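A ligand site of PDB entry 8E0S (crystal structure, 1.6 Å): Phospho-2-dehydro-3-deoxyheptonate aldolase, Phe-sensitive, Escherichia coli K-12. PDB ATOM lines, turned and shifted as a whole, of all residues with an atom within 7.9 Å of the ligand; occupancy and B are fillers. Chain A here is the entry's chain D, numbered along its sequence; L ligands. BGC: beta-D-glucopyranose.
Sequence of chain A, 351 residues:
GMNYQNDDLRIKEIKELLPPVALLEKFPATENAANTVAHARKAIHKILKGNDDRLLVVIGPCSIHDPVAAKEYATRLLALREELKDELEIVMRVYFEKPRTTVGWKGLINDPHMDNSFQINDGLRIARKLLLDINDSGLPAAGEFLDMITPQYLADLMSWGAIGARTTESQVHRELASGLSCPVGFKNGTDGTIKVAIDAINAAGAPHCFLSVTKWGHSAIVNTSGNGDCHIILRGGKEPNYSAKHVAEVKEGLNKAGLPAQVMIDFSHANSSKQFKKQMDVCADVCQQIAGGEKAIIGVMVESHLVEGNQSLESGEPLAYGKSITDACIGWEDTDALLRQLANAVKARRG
O of Leu 306 lies within hydrogen-bond range of O1 of the ligand (2.6 Å). The guanidinium group of Arg 76 sits at hydrogen-bond distance from an oxygen (O6) of the ligand. The side-chain carboxylate (OE2) of Glu 72 is in hydrogen-bond range of an oxygen (O6) of the ligand.
O of Leu 306 lies within hydrogen-bond range of N of Trp 332 (3.0 Å). The guanidinium group of Arg 76 is in salt-bridge range of the side-chain carboxylate of Glu 72 (2.9 Å). The side-chain hydroxyl of Tyr 321 lies within hydrogen-bond range of the side-chain carboxylate of Glu 72 (2.5 Å). O of His 305 lies within hydrogen-bond range of N of Trp 332 (3.3 Å).
Merely in contact with the ligand: Tyr 321 (3.9 Å) and Trp 332 (3.3 Å). Within 4 Å of the ligand: Glu 72, Arg 76, Leu 306, Tyr 321 and Trp 332.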
ATOM      1  N   ALA A  69      14.636  -3.550  25.477  1.00  0.00           N
ATOM      2  CA  ALA A  69      13.468  -2.673  25.556  1.00  0.00           C
ATOM      3  C   ALA A  69      12.485  -2.948  24.422  1.00  0.00           C
ATOM      4  O   ALA A  69      11.257  -2.855  24.609  1.00  0.00           O
ATOM      5  CB  ALA A  69      13.917  -1.206  25.521  1.00  0.00           C
ATOM      6  N   GLU A  72      10.397  -5.930  25.530  1.00  0.00           N
ATOM      7  CA  GLU A  72       9.414  -5.534  26.544  1.00  0.00           C
ATOM      8  C   GLU A  72       8.255  -4.754  25.914  1.00  0.00           C
ATOM      9  O   GLU A  72       7.081  -4.982  26.231  1.00  0.00           O
ATOM     10  CB  GLU A  72      10.080  -4.707  27.641  1.00  0.00           C
ATOM     11  CG  GLU A  72       9.054  -4.151  28.613  1.00  0.00           C
ATOM     12  CD  GLU A  72       9.649  -3.569  29.872  1.00  0.00           C
ATOM     13  OE1 GLU A  72      10.885  -3.460  29.976  1.00  0.00           O
ATOM     14  OE2 GLU A  72       8.857  -3.206  30.780  1.00  0.00           O
ATOM     15  N   TYR A  73       8.581  -3.837  24.992  1.00  0.00           N
ATOM     16  CA  TYR A  73       7.534  -3.097  24.288  1.00  0.00           C
ATOM     17  C   TYR A  73       6.643  -4.057  23.517  1.00  0.00           C
ATOM     18  O   TYR A  73       5.413  -3.919  23.528  1.00  0.00           O
ATOM     19  CB  TYR A  73       8.161  -2.074  23.344  1.00  0.00           C
ATOM     20  CG  TYR A  73       7.143  -1.207  22.618  1.00  0.00           C
ATOM     21  CD1 TYR A  73       6.546  -1.620  21.420  1.00  0.00           C
ATOM     22  CD2 TYR A  73       6.777   0.039  23.128  1.00  0.00           C
ATOM     23  CE1 TYR A  73       5.604  -0.846  20.779  1.00  0.00           C
ATOM     24  CE2 TYR A  73       5.820   0.831  22.480  1.00  0.00           C
ATOM     25  CZ  TYR A  73       5.271   0.403  21.282  1.00  0.00           C
ATOM     26  OH  TYR A  73       4.334   1.171  20.629  1.00  0.00           O
ATOM     27  N   ARG A  76       4.089  -5.751  25.807  1.00  0.00           N
ATOM     28  CA  ARG A  76       2.971  -4.872  26.122  1.00  0.00           C
ATOM     29  C   ARG A  76       2.064  -4.676  24.926  1.00  0.00           C
ATOM     30  O   ARG A  76       0.839  -4.638  25.076  1.00  0.00           O
ATOM     31  CB  ARG A  76       3.496  -3.519  26.596  1.00  0.00           C
ATOM     32  CG  ARG A  76       4.350  -3.603  27.831  1.00  0.00           C
ATOM     33  CD  ARG A  76       4.365  -2.251  28.515  1.00  0.00           C
ATOM     34  NE  ARG A  76       5.440  -2.160  29.477  1.00  0.00           N
ATOM     35  CZ  ARG A  76       5.875  -1.011  29.976  1.00  0.00           C
ATOM     36  NH1 ARG A  76       5.296   0.143  29.652  1.00  0.00           N
ATOM     37  NH2 ARG A  76       6.907  -1.016  30.822  1.00  0.00           N
ATOM     38  N   HIS A 305       7.089   4.516  22.409  1.00  0.00           N
ATOM     39  CA  HIS A 305       8.097   3.712  23.090  1.00  0.00           C
ATOM     40  C   HIS A 305       7.623   3.485  24.525  1.00  0.00           C
ATOM     41  O   HIS A 305       6.571   3.972  24.920  1.00  0.00           O
ATOM     42  CB  HIS A 305       9.454   4.408  23.044  1.00  0.00           C
ATOM     43  CG  HIS A 305      10.597   3.453  22.888  1.00  0.00           C
ATOM     44  ND1 HIS A 305      10.627   2.226  23.523  1.00  0.00           N
ATOM     45  CD2 HIS A 305      11.756   3.553  22.196  1.00  0.00           C
ATOM     46  CE1 HIS A 305      11.761   1.622  23.228  1.00  0.00           C
ATOM     47  NE2 HIS A 305      12.462   2.393  22.427  1.00  0.00           N
ATOM     48  N   LEU A 306       8.395   2.705  25.284  1.00  0.00           N
ATOM     49  CA  LEU A 306       8.070   2.494  26.697  1.00  0.00           C
ATOM     50  C   LEU A 306       8.020   3.821  27.430  1.00  0.00           C
ATOM     51  O   LEU A 306       7.087   4.100  28.205  1.00  0.00           O
ATOM     52  CB  LEU A 306       9.098   1.572  27.356  1.00  0.00           C
ATOM     53  CG  LEU A 306       9.176   0.161  26.779  1.00  0.00           C
ATOM     54  CD1 LEU A 306      10.283  -0.663  27.422  1.00  0.00           C
ATOM     55  CD2 LEU A 306       7.852  -0.529  26.976  1.00  0.00           C
ATOM     56  N   VAL A 307       9.049   4.634  27.230  1.00  0.00           N
ATOM     57  CA  VAL A 307       9.248   5.892  27.946  1.00  0.00           C
ATOM     58  C   VAL A 307       9.208   6.988  26.915  1.00  0.00           C
ATOM     59  O   VAL A 307       9.828   6.868  25.842  1.00  0.00           O
ATOM     60  CB  VAL A 307      10.579   5.861  28.721  1.00  0.00           C
ATOM     61  CG1 VAL A 307      10.886   7.237  29.347  1.00  0.00           C
ATOM     62  CG2 VAL A 307      10.584   4.708  29.753  1.00  0.00           C
ATOM     63  N   GLU A 308       8.435   8.047  27.192  1.00  0.00           N
ATOM     64  CA  GLU A 308       8.223   9.106  26.227  1.00  0.00           C
ATOM     65  C   GLU A 308       9.483   9.954  26.049  1.00  0.00           C
ATOM     66  O   GLU A 308      10.431   9.880  26.835  1.00  0.00           O
ATOM     67  CB  GLU A 308       7.080  10.018  26.675  1.00  0.00           C
ATOM     68  CG  GLU A 308       7.497  10.959  27.823  1.00  0.00           C
ATOM     69  CD  GLU A 308       6.344  11.776  28.368  1.00  0.00           C
ATOM     70  OE1 GLU A 308       5.257  11.828  27.729  1.00  0.00           O
ATOM     71  OE2 GLU A 308       6.531  12.360  29.470  1.00  0.00           O
ATOM     72  N   TYR A 321      16.636   3.737  29.886  1.00  0.00           N
ATOM     73  CA  TYR A 321      16.009   2.555  29.327  1.00  0.00           C
ATOM     74  C   TYR A 321      14.682   2.907  28.669  1.00  0.00           C
ATOM     75  O   TYR A 321      13.920   3.726  29.170  1.00  0.00           O
ATOM     76  CB  TYR A 321      15.795   1.514  30.422  1.00  0.00           C
ATOM     77  CG  TYR A 321      15.084   0.263  29.971  1.00  0.00           C
ATOM     78  CD1 TYR A 321      15.767  -0.754  29.319  1.00  0.00           C
ATOM     79  CD2 TYR A 321      13.734   0.081  30.242  1.00  0.00           C
ATOM     80  CE1 TYR A 321      15.125  -1.917  28.921  1.00  0.00           C
ATOM     81  CE2 TYR A 321      13.068  -1.084  29.862  1.00  0.00           C
ATOM     82  CZ  TYR A 321      13.790  -2.084  29.199  1.00  0.00           C
ATOM     83  OH  TYR A 321      13.143  -3.240  28.812  1.00  0.00           O
ATOM     84  N   GLY A 322      14.449   2.302  27.503  1.00  0.00           N
ATOM     85  CA  GLY A 322      13.149   2.416  26.871  1.00  0.00           C
ATOM     86  C   GLY A 322      12.813   3.771  26.285  1.00  0.00           C
ATOM     87  O   GLY A 322      11.648   4.033  26.035  1.00  0.00           O
ATOM     88  N   GLY A 331       5.011   7.809  25.164  1.00  0.00           N
ATOM     89  CA  GLY A 331       5.341   6.722  26.060  1.00  0.00           C
ATOM     90  C   GLY A 331       4.168   5.780  26.218  1.00  0.00           C
ATOM     91  O   GLY A 331       3.136   5.915  25.547  1.00  0.00           O
ATOM     92  N   TRP A 332       4.325   4.822  27.135  1.00  0.00           N
ATOM     93  CA  TRP A 332       3.364   3.712  27.139  1.00  0.00           C
ATOM     94  C   TRP A 332       1.985   4.186  27.591  1.00  0.00           C
ATOM     95  O   TRP A 332       0.975   3.812  26.970  1.00  0.00           O
ATOM     96  CB  TRP A 332       3.860   2.536  27.983  1.00  0.00           C
ATOM     97  CG  TRP A 332       2.895   1.439  27.761  1.00  0.00           C
ATOM     98  CD1 TRP A 332       1.909   1.033  28.610  1.00  0.00           C
ATOM     99  CD2 TRP A 332       2.729   0.682  26.556  1.00  0.00           C
ATOM    100  NE1 TRP A 332       1.145   0.042  28.010  1.00  0.00           N
ATOM    101  CE2 TRP A 332       1.645  -0.194  26.754  1.00  0.00           C
ATOM    102  CE3 TRP A 332       3.418   0.637  25.334  1.00  0.00           C
ATOM    103  CZ2 TRP A 332       1.215  -1.093  25.764  1.00  0.00           C
ATOM    104  CZ3 TRP A 332       2.997  -0.262  24.356  1.00  0.00           C
ATOM    105  CH2 TRP A 332       1.902  -1.114  24.570  1.00  0.00           C
ATOM    106  N   GLU A 333       1.911   5.032  28.620  1.00  0.00           N
ATOM    107  CA  GLU A 333       0.594   5.503  29.087  1.00  0.00           C
ATOM    108  C   GLU A 333      -0.218   6.131  27.965  1.00  0.00           C
ATOM    109  O   GLU A 333      -1.373   5.763  27.751  1.00  0.00           O
ATOM    110  CB  GLU A 333       0.754   6.477  30.250  1.00  0.00           C
ATOM    111  CG  GLU A 333      -0.572   6.884  30.866  1.00  0.00           C
ATOM    112  CD  GLU A 333      -1.166   5.836  31.785  1.00  0.00           C
ATOM    113  OE1 GLU A 333      -0.426   4.995  32.312  1.00  0.00           O
ATOM    114  OE2 GLU A 333      -2.402   5.881  31.977  1.00  0.00           O
ATOM    115  N   ASP A 334       0.374   7.079  27.216  1.00  0.00           N
ATOM    116  CA  ASP A 334      -0.307   7.672  26.076  1.00  0.00           C
ATOM    117  C   ASP A 334      -0.600   6.643  24.977  1.00  0.00           C
ATOM    118  O   ASP A 334      -1.586   6.765  24.254  1.00  0.00           O
ATOM    119  CB  ASP A 334       0.520   8.802  25.467  1.00  0.00           C
ATOM    120  CG  ASP A 334       0.344  10.129  26.187  1.00  0.00           C
ATOM    121  OD1 ASP A 334      -0.674  10.288  26.886  1.00  0.00           O
ATOM    122  OD2 ASP A 334       1.231  11.002  26.021  1.00  0.00           O
HETATM  123  C2  BGC L   1       6.685   3.092  32.633  1.00  0.00           C
HETATM  124  C3  BGC L   1       7.765   2.973  33.691  1.00  0.00           C
HETATM  125  C4  BGC L   1       8.543   1.692  33.475  1.00  0.00           C
HETATM  126  C5  BGC L   1       9.119   1.723  32.054  1.00  0.00           C
HETATM  127  C6  BGC L   1      10.042   0.551  31.790  1.00  0.00           C
HETATM  128  C1  BGC L   1       7.254   2.897  31.229  1.00  0.00           C
HETATM  129  O1  BGC L   1       6.172   2.804  30.307  1.00  0.00           O
HETATM  130  O2  BGC L   1       6.078   4.381  32.723  1.00  0.00           O
HETATM  131  O3  BGC L   1       7.161   2.976  34.983  1.00  0.00           O
HETATM  132  O4  BGC L   1       9.581   1.590  34.450  1.00  0.00           O
HETATM  133  O5  BGC L   1       8.012   1.691  31.158  1.00  0.00           O
HETATM  134  O6  BGC L   1       9.390  -0.676  32.095  1.00  0.00           O
